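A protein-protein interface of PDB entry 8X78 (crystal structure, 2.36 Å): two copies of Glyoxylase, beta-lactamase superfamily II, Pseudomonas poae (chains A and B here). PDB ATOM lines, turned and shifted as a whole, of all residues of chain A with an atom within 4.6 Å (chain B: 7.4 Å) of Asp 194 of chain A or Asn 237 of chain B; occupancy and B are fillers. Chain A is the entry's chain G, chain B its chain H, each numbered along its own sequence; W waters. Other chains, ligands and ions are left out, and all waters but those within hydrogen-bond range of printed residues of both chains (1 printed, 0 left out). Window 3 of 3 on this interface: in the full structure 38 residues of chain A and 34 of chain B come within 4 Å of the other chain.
N of Ala 238 of chain B sits at hydrogen-bond distance from O of Gly 236 of chain A (2.8 Å).
The backbone carbonyl oxygen of Gly 236 of chain A lies close to the backbone carbonyl oxygen of Gly 236 of chain B.
The side-chain carboxylate of Asp 194 of chain A is in salt-bridge range of the side-chain amino group of Lys 193 of chain A (3.5 Å).
The backbone NH of Asn 240 of chain A is in hydrogen-bond range of the side-chain amide oxygen of Asn 237 of chain A, at 3.0 Å.
The backbone carbonyl oxygen (O) of Asp 194 of chain B sits at hydrogen-bond distance from the backbone NH (N) of Asn 237 of chain B.
The side-chain amide nitrogen of Asn 240 of chain B sits at hydrogen-bond distance from the backbone carbonyl oxygen of Asp 194 of chain B (3.0 Å).
The backbone NH (N) of Asn 237 of chain B sits at hydrogen-bond distance from the backbone carbonyl oxygen (O) of Ser 195 of chain B (3.2 Å).
The side-chain amide oxygen (OD1) of Asn 237 of chain B is in hydrogen-bond range of the backbone NH (N) of Phe 239 of chain B (2.7 Å).
ND2 of Asn 237 of chain B touches CB of Asp 194 of chain A, 3.8 Å away.
Phe 239 of chain B touches Phe 198 of chain A (CD2 to CZ, 3.4 Å).
Gly 236 of chain A touches Asn 237 of chain B.
Asn 237 of chain A touches Asp 194 of chain B (ND2 to CB, 3.8 Å).
Asn 237 of chain A touches Gly 236 of chain B (CA to O, 3.2 Å).
CA of Asn 237 of chain A touches CA of Asn 237 of chain B, at 3.9 Å.
Asp 194 of chain A touches one residue of chain B.
Of the printed residues of chain B, Asn 237 of chain A touches Asp 194 (3.8 Å), Gly 236 (3.2 Å) and Asn 237 (3.9 Å).
Of the printed residues of chain A, Asn 237 of chain B touches Asp 194 (3.8 Å), Gly 236 (3.2 Å) and Asn 237 (3.9 Å).
Of the printed residues of chain A, Ala 238 of chain B touches Gly 236 (2.8 Å).
Of the printed residues of chain A, Phe 239 of chain B touches Phe 198.
The nearest printed residue of chain B that does not touch Asp 194 of chain A is Asn 240 of chain B (6.6 Å).
The nearest printed residue of chain A that does not touch Asp 194 of chain B is Asn 240 of chain A (6.4 Å).
Among the printed residues, 8 pairs touch across the chains.
Asp 194 of chain A touches Asn 237 of chain B, and with the chains exchanged Asn 237 of chain A touches Asp 194 of chain B.
Gly 236 of chain B touches its own counterpart, Gly 236 of chain A.
Gly 236 of chain A touches Asn 237 of chain B, and with the chains exchanged Asn 237 of chain A touches Gly 236 of chain B.
Asn 237 of chain B touches its own counterpart, Asn 237 of chain A.
Positions printed for both chains: 193, 194, 195, 196, 197, 198, 236, 237 and 240.
Of the 8 pairs that touch across the chains among the printed residues, 6 have their exchanged pair printed and touching as well.
Water W1 lies within hydrogen-bond range of OD1 of Asp 194 of chain B and ND2 of Asn 237 of chain A.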
ATOM      1  N   ALA A 192     -35.031  -3.038   0.031  1.00  0.00           N
ATOM      2  CA  ALA A 192     -33.779  -3.762  -0.207  1.00  0.00           C
ATOM      3  C   ALA A 192     -33.455  -4.485   1.091  1.00  0.00           C
ATOM      4  O   ALA A 192     -32.595  -4.058   1.864  1.00  0.00           O
ATOM      5  CB  ALA A 192     -32.638  -2.826  -0.633  1.00  0.00           C
ATOM      6  N   LYS A 193     -34.151  -5.590   1.319  1.00  0.00           N
ATOM      7  CA  LYS A 193     -34.056  -6.304   2.584  1.00  0.00           C
ATOM      8  C   LYS A 193     -32.625  -6.778   2.831  1.00  0.00           C
ATOM      9  O   LYS A 193     -31.982  -7.352   1.945  1.00  0.00           O
ATOM     10  CB  LYS A 193     -35.031  -7.493   2.574  1.00  0.00           C
ATOM     11  CG  LYS A 193     -35.278  -8.074   3.962  1.00  0.00           C
ATOM     12  CD  LYS A 193     -36.397  -9.117   3.967  1.00  0.00           C
ATOM     13  CE  LYS A 193     -36.678  -9.592   5.402  1.00  0.00           C
ATOM     14  NZ  LYS A 193     -35.793 -10.725   5.781  1.00  0.00           N
ATOM     15  N   ASP A 194     -32.120  -6.525   4.037  1.00  0.00           N
ATOM     16  CA  ASP A 194     -30.795  -6.994   4.427  1.00  0.00           C
ATOM     17  C   ASP A 194     -29.741  -6.556   3.420  1.00  0.00           C
ATOM     18  O   ASP A 194     -28.831  -7.309   3.074  1.00  0.00           O
ATOM     19  CB  ASP A 194     -30.776  -8.515   4.590  1.00  0.00           C
ATOM     20  CG  ASP A 194     -31.814  -8.997   5.593  1.00  0.00           C
ATOM     21  OD1 ASP A 194     -32.008  -8.312   6.644  1.00  0.00           O
ATOM     22  OD2 ASP A 194     -32.438 -10.050   5.325  1.00  0.00           O
ATOM     23  N   SER A 195     -29.835  -5.310   2.983  1.00  0.00           N
ATOM     24  CA  SER A 195     -28.822  -4.747   2.104  1.00  0.00           C
ATOM     25  C   SER A 195     -27.850  -3.939   2.955  1.00  0.00           C
ATOM     26  O   SER A 195     -26.887  -4.498   3.495  1.00  0.00           O
ATOM     27  CB  SER A 195     -29.475  -3.897   1.010  1.00  0.00           C
ATOM     28  OG  SER A 195     -30.411  -2.964   1.562  1.00  0.00           O
ATOM     29  N   HIS A 196     -28.083  -2.629   3.078  1.00  0.00           N
ATOM     30  CA  HIS A 196     -27.322  -1.844   4.049  1.00  0.00           C
ATOM     31  C   HIS A 196     -27.768  -2.116   5.491  1.00  0.00           C
ATOM     32  O   HIS A 196     -26.941  -2.103   6.413  1.00  0.00           O
ATOM     33  CB  HIS A 196     -27.425  -0.364   3.732  1.00  0.00           C
ATOM     34  CG  HIS A 196     -26.551   0.467   4.602  1.00  0.00           C
ATOM     35  ND1 HIS A 196     -27.051   1.368   5.525  1.00  0.00           N
ATOM     36  CD2 HIS A 196     -25.204   0.508   4.719  1.00  0.00           C
ATOM     37  CE1 HIS A 196     -26.043   1.937   6.157  1.00  0.00           C
ATOM     38  NE2 HIS A 196     -24.913   1.437   5.686  1.00  0.00           N
ATOM     39  N   THR A 197     -29.071  -2.315   5.708  1.00  0.00           N
ATOM     40  CA  THR A 197     -29.633  -2.632   7.018  1.00  0.00           C
ATOM     41  C   THR A 197     -30.829  -3.550   6.793  1.00  0.00           C
ATOM     42  O   THR A 197     -31.220  -3.811   5.651  1.00  0.00           O
ATOM     43  CB  THR A 197     -30.080  -1.376   7.786  1.00  0.00           C
ATOM     44  OG1 THR A 197     -31.168  -0.742   7.090  1.00  0.00           O
ATOM     45  CG2 THR A 197     -28.945  -0.408   7.868  1.00  0.00           C
ATOM     46  N   PHE A 198     -31.438  -3.996   7.895  1.00  0.00           N
ATOM     47  CA  PHE A 198     -32.561  -4.933   7.832  1.00  0.00           C
ATOM     48  C   PHE A 198     -33.585  -4.540   6.784  1.00  0.00           C
ATOM     49  O   PHE A 198     -33.992  -5.360   5.955  1.00  0.00           O
ATOM     50  CB  PHE A 198     -33.235  -5.043   9.193  1.00  0.00           C
ATOM     51  CG  PHE A 198     -32.298  -5.407  10.287  1.00  0.00           C
ATOM     52  CD1 PHE A 198     -31.761  -6.697  10.340  1.00  0.00           C
ATOM     53  CD2 PHE A 198     -31.939  -4.469  11.256  1.00  0.00           C
ATOM     54  CE1 PHE A 198     -30.878  -7.053  11.340  1.00  0.00           C
ATOM     55  CE2 PHE A 198     -31.071  -4.812  12.270  1.00  0.00           C
ATOM     56  CZ  PHE A 198     -30.527  -6.110  12.311  1.00  0.00           C
ATOM     57  N   GLY A 236     -25.597  -5.175   6.665  1.00  0.00           N
ATOM     58  CA  GLY A 236     -26.432  -6.120   5.944  1.00  0.00           C
ATOM     59  C   GLY A 236     -25.629  -7.150   5.173  1.00  0.00           C
ATOM     60  O   GLY A 236     -24.594  -7.637   5.648  1.00  0.00           O
ATOM     61  N   ASN A 237     -26.091  -7.468   3.963  1.00  0.00           N
ATOM     62  CA  ASN A 237     -25.549  -8.547   3.145  1.00  0.00           C
ATOM     63  C   ASN A 237     -24.865  -7.924   1.929  1.00  0.00           C
ATOM     64  O   ASN A 237     -25.514  -7.266   1.106  1.00  0.00           O
ATOM     65  CB  ASN A 237     -26.654  -9.512   2.716  1.00  0.00           C
ATOM     66  CG  ASN A 237     -26.122 -10.678   1.850  1.00  0.00           C
ATOM     67  OD1 ASN A 237     -25.319 -10.471   0.936  1.00  0.00           O
ATOM     68  ND2 ASN A 237     -26.596 -11.893   2.121  1.00  0.00           N
ATOM     69  N   ASN A 240     -26.367  -8.863  -1.340  1.00  0.00           N
ATOM     70  CA  ASN A 240     -27.637  -8.174  -1.565  1.00  0.00           C
ATOM     71  C   ASN A 240     -27.403  -6.790  -2.152  1.00  0.00           C
ATOM     72  O   ASN A 240     -28.142  -6.352  -3.039  1.00  0.00           O
ATOM     73  CB  ASN A 240     -28.446  -8.053  -0.271  1.00  0.00           C
ATOM     74  CG  ASN A 240     -29.134  -9.345   0.123  1.00  0.00           C
ATOM     75  OD1 ASN A 240     -28.986 -10.360  -0.539  1.00  0.00           O
ATOM     76  ND2 ASN A 240     -29.899  -9.304   1.214  1.00  0.00           N
ATOM     77  N   LYS B 193     -26.007 -19.901   6.893  1.00  0.00           N
ATOM     78  CA  LYS B 193     -26.398 -19.286   5.634  1.00  0.00           C
ATOM     79  C   LYS B 193     -26.128 -17.781   5.655  1.00  0.00           C
ATOM     80  O   LYS B 193     -26.471 -17.075   6.616  1.00  0.00           O
ATOM     81  CB  LYS B 193     -27.878 -19.567   5.346  1.00  0.00           C
ATOM     82  CG  LYS B 193     -28.311 -19.221   3.917  1.00  0.00           C
ATOM     83  CD  LYS B 193     -29.768 -19.617   3.645  1.00  0.00           C
ATOM     84  CE  LYS B 193     -30.056 -19.762   2.130  1.00  0.00           C
ATOM     85  NZ  LYS B 193     -30.013 -18.484   1.325  1.00  0.00           N
ATOM     86  N   ASP B 194     -25.497 -17.293   4.588  1.00  0.00           N
ATOM     87  CA  ASP B 194     -25.224 -15.867   4.430  1.00  0.00           C
ATOM     88  C   ASP B 194     -24.417 -15.301   5.601  1.00  0.00           C
ATOM     89  O   ASP B 194     -24.746 -14.253   6.141  1.00  0.00           O
ATOM     90  CB  ASP B 194     -26.522 -15.080   4.251  1.00  0.00           C
ATOM     91  CG  ASP B 194     -27.329 -15.561   3.064  1.00  0.00           C
ATOM     92  OD1 ASP B 194     -26.727 -15.776   1.988  1.00  0.00           O
ATOM     93  OD2 ASP B 194     -28.557 -15.755   3.205  1.00  0.00           O
ATOM     94  N   SER B 195     -23.338 -15.990   5.977  1.00  0.00           N
ATOM     95  CA  SER B 195     -22.393 -15.445   6.944  1.00  0.00           C
ATOM     96  C   SER B 195     -21.161 -14.880   6.223  1.00  0.00           C
ATOM     97  O   SER B 195     -21.236 -13.751   5.722  1.00  0.00           O
ATOM     98  CB  SER B 195     -22.024 -16.508   7.979  1.00  0.00           C
ATOM     99  OG  SER B 195     -21.855 -17.776   7.382  1.00  0.00           O
ATOM    100  N   HIS B 196     -20.025 -15.612   6.169  1.00  0.00           N
ATOM    101  CA  HIS B 196     -18.929 -15.187   5.284  1.00  0.00           C
ATOM    102  C   HIS B 196     -19.372 -15.293   3.837  1.00  0.00           C
ATOM    103  O   HIS B 196     -19.049 -14.426   3.016  1.00  0.00           O
ATOM    104  CB  HIS B 196     -17.623 -16.003   5.491  1.00  0.00           C
ATOM    105  CG  HIS B 196     -16.384 -15.351   4.903  1.00  0.00           C
ATOM    106  ND1 HIS B 196     -15.439 -15.986   4.082  1.00  0.00           N
ATOM    107  CD2 HIS B 196     -15.946 -14.081   5.054  1.00  0.00           C
ATOM    108  CE1 HIS B 196     -14.499 -15.114   3.765  1.00  0.00           C
ATOM    109  NE2 HIS B 196     -14.780 -13.961   4.339  1.00  0.00           N
ATOM    110  N   THR B 197     -20.112 -16.354   3.504  1.00  0.00           N
ATOM    111  CA  THR B 197     -20.541 -16.596   2.135  1.00  0.00           C
ATOM    112  C   THR B 197     -21.930 -17.207   2.148  1.00  0.00           C
ATOM    113  O   THR B 197     -22.479 -17.534   3.200  1.00  0.00           O
ATOM    114  CB  THR B 197     -19.571 -17.521   1.376  1.00  0.00           C
ATOM    115  OG1 THR B 197     -19.583 -18.828   1.970  1.00  0.00           O
ATOM    116  CG2 THR B 197     -18.173 -16.976   1.416  1.00  0.00           C
ATOM    117  N   PHE B 198     -22.480 -17.373   0.943  1.00  0.00           N
ATOM    118  CA  PHE B 198     -23.826 -17.902   0.757  1.00  0.00           C
ATOM    119  C   PHE B 198     -24.128 -19.078   1.688  1.00  0.00           C
ATOM    120  O   PHE B 198     -25.166 -19.117   2.356  1.00  0.00           O
ATOM    121  CB  PHE B 198     -24.005 -18.346  -0.700  1.00  0.00           C
ATOM    122  CG  PHE B 198     -23.751 -17.263  -1.722  1.00  0.00           C
ATOM    123  CD1 PHE B 198     -24.599 -16.163  -1.829  1.00  0.00           C
ATOM    124  CD2 PHE B 198     -22.679 -17.379  -2.613  1.00  0.00           C
ATOM    125  CE1 PHE B 198     -24.375 -15.193  -2.789  1.00  0.00           C
ATOM    126  CE2 PHE B 198     -22.437 -16.416  -3.569  1.00  0.00           C
ATOM    127  CZ  PHE B 198     -23.283 -15.321  -3.663  1.00  0.00           C
ATOM    128  N   PRO B 230     -17.864  -7.544  12.950  1.00  0.00           N
ATOM    129  CA  PRO B 230     -17.628  -8.245  11.679  1.00  0.00           C
ATOM    130  C   PRO B 230     -16.536  -7.561  10.873  1.00  0.00           C
ATOM    131  O   PRO B 230     -16.293  -6.355  11.036  1.00  0.00           O
ATOM    132  CB  PRO B 230     -18.988  -8.180  10.965  1.00  0.00           C
ATOM    133  CG  PRO B 230     -19.761  -7.063  11.678  1.00  0.00           C
ATOM    134  CD  PRO B 230     -19.218  -6.964  13.064  1.00  0.00           C
ATOM    135  N   HIS B 234     -16.079  -9.113   3.537  1.00  0.00           N
ATOM    136  CA  HIS B 234     -16.725 -10.418   3.617  1.00  0.00           C
ATOM    137  C   HIS B 234     -17.782 -10.432   2.526  1.00  0.00           C
ATOM    138  O   HIS B 234     -18.005  -9.430   1.839  1.00  0.00           O
ATOM    139  CB  HIS B 234     -17.305 -10.689   5.006  1.00  0.00           C
ATOM    140  CG  HIS B 234     -18.458  -9.807   5.364  1.00  0.00           C
ATOM    141  ND1 HIS B 234     -19.713  -9.956   4.808  1.00  0.00           N
ATOM    142  CD2 HIS B 234     -18.549  -8.762   6.222  1.00  0.00           C
ATOM    143  CE1 HIS B 234     -20.527  -9.041   5.308  1.00  0.00           C
ATOM    144  NE2 HIS B 234     -19.844  -8.306   6.168  1.00  0.00           N
ATOM    145  N   GLN B 235     -18.431 -11.576   2.352  1.00  0.00           N
ATOM    146  CA  GLN B 235     -19.361 -11.671   1.235  1.00  0.00           C
ATOM    147  C   GLN B 235     -20.698 -12.263   1.668  1.00  0.00           C
ATOM    148  O   GLN B 235     -21.365 -12.939   0.881  1.00  0.00           O
ATOM    149  CB  GLN B 235     -18.724 -12.441   0.077  1.00  0.00           C
ATOM    150  CG  GLN B 235     -17.421 -11.769  -0.427  1.00  0.00           C
ATOM    151  CD  GLN B 235     -16.833 -12.399  -1.686  1.00  0.00           C
ATOM    152  OE1 GLN B 235     -16.435 -13.566  -1.688  1.00  0.00           O
ATOM    153  NE2 GLN B 235     -16.774 -11.624  -2.763  1.00  0.00           N
ATOM    154  N   GLY B 236     -21.109 -11.981   2.907  1.00  0.00           N
ATOM    155  CA  GLY B 236     -22.435 -12.298   3.406  1.00  0.00           C
ATOM    156  C   GLY B 236     -23.026 -11.227   4.309  1.00  0.00           C
ATOM    157  O   GLY B 236     -22.894 -10.020   4.049  1.00  0.00           O
ATOM    158  N   ASN B 237     -23.668 -11.645   5.392  1.00  0.00           N
ATOM    159  CA  ASN B 237     -24.513 -10.756   6.179  1.00  0.00           C
ATOM    160  C   ASN B 237     -23.857 -10.415   7.516  1.00  0.00           C
ATOM    161  O   ASN B 237     -23.681 -11.288   8.374  1.00  0.00           O
ATOM    162  CB  ASN B 237     -25.891 -11.371   6.400  1.00  0.00           C
ATOM    163  CG  ASN B 237     -26.825 -10.427   7.147  1.00  0.00           C
ATOM    164  OD1 ASN B 237     -26.430  -9.827   8.155  1.00  0.00           O
ATOM    165  ND2 ASN B 237     -28.045 -10.262   6.645  1.00  0.00           N
ATOM    166  N   ALA B 238     -23.537  -9.134   7.702  1.00  0.00           N
ATOM    167  CA  ALA B 238     -22.886  -8.684   8.933  1.00  0.00           C
ATOM    168  C   ALA B 238     -23.653  -9.127  10.173  1.00  0.00           C
ATOM    169  O   ALA B 238     -23.074  -9.703  11.101  1.00  0.00           O
ATOM    170  CB  ALA B 238     -22.746  -7.164   8.927  1.00  0.00           C
ATOM    171  N   PHE B 239     -24.967  -8.876  10.208  1.00  0.00           N
ATOM    172  CA  PHE B 239     -25.726  -9.278  11.389  1.00  0.00           C
ATOM    173  C   PHE B 239     -25.831 -10.793  11.524  1.00  0.00           C
ATOM    174  O   PHE B 239     -25.852 -11.297  12.652  1.00  0.00           O
ATOM    175  CB  PHE B 239     -27.101  -8.627  11.389  1.00  0.00           C
ATOM    176  CG  PHE B 239     -27.174  -7.402  12.264  1.00  0.00           C
ATOM    177  CD1 PHE B 239     -27.229  -7.521  13.643  1.00  0.00           C
ATOM    178  CD2 PHE B 239     -27.173  -6.132  11.708  1.00  0.00           C
ATOM    179  CE1 PHE B 239     -27.298  -6.382  14.454  1.00  0.00           C
ATOM    180  CE2 PHE B 239     -27.249  -5.000  12.504  1.00  0.00           C
ATOM    181  CZ  PHE B 239     -27.303  -5.118  13.876  1.00  0.00           C
ATOM    182  N   ASN B 240     -25.872 -11.538  10.406  1.00  0.00           N
ATOM    183  CA  ASN B 240     -25.801 -12.996  10.500  1.00  0.00           C
ATOM    184  C   ASN B 240     -24.517 -13.445  11.184  1.00  0.00           C
ATOM    185  O   ASN B 240     -24.522 -14.394  11.979  1.00  0.00           O
ATOM    186  CB  ASN B 240     -25.898 -13.628   9.115  1.00  0.00           C
ATOM    187  CG  ASN B 240     -27.302 -13.664   8.611  1.00  0.00           C
ATOM    188  OD1 ASN B 240     -28.201 -13.180   9.283  1.00  0.00           O
ATOM    189  ND2 ASN B 240     -27.507 -14.219   7.427  1.00  0.00           N
ATOM    190  N   GLN B 241     -23.395 -12.790  10.879  1.00  0.00           N
ATOM    191  CA  GLN B 241     -22.165 -13.157  11.565  1.00  0.00           C
ATOM    192  C   GLN B 241     -22.274 -12.890  13.057  1.00  0.00           C
ATOM    193  O   GLN B 241     -21.831 -13.707  13.872  1.00  0.00           O
ATOM    194  CB  GLN B 241     -20.982 -12.419  10.954  1.00  0.00           C
ATOM    195  CG  GLN B 241     -20.500 -13.095   9.711  1.00  0.00           C
ATOM    196  CD  GLN B 241     -19.585 -12.221   8.920  1.00  0.00           C
ATOM    197  OE1 GLN B 241     -20.017 -11.550   7.966  1.00  0.00           O
ATOM    198  NE2 GLN B 241     -18.304 -12.217   9.293  1.00  0.00           N
ATOM    199  N   ILE B 242     -22.890 -11.765  13.433  1.00  0.00           N
ATOM    200  CA  ILE B 242     -23.090 -11.465  14.845  1.00  0.00           C
ATOM    201  C   ILE B 242     -23.836 -12.616  15.515  1.00  0.00           C
ATOM    202  O   ILE B 242     -23.460 -13.073  16.601  1.00  0.00           O
ATOM    203  CB  ILE B 242     -23.817 -10.108  14.993  1.00  0.00           C
ATOM    204  CG1 ILE B 242     -22.837  -8.944  14.747  1.00  0.00           C
ATOM    205  CG2 ILE B 242     -24.557  -9.981  16.342  1.00  0.00           C
ATOM    206  CD1 ILE B 242     -21.878  -8.667  15.919  1.00  0.00           C
ATOM    207  N   ASP B 243     -24.870 -13.146  14.850  1.00  0.00           N
ATOM    208  CA  ASP B 243     -25.636 -14.242  15.448  1.00  0.00           C
ATOM    209  C   ASP B 243     -24.865 -15.568  15.439  1.00  0.00           C
ATOM    210  O   ASP B 243     -25.051 -16.396  16.340  1.00  0.00           O
ATOM    211  CB  ASP B 243     -26.991 -14.369  14.749  1.00  0.00           C
ATOM    212  CG  ASP B 243     -27.949 -13.230  15.135  1.00  0.00           C
ATOM    213  OD1 ASP B 243     -28.068 -12.946  16.350  1.00  0.00           O
ATOM    214  OD2 ASP B 243     -28.563 -12.600  14.238  1.00  0.00           O
HETATM  215  O   HOH W   1     -26.165 -13.885   0.210  1.00  0.00           O
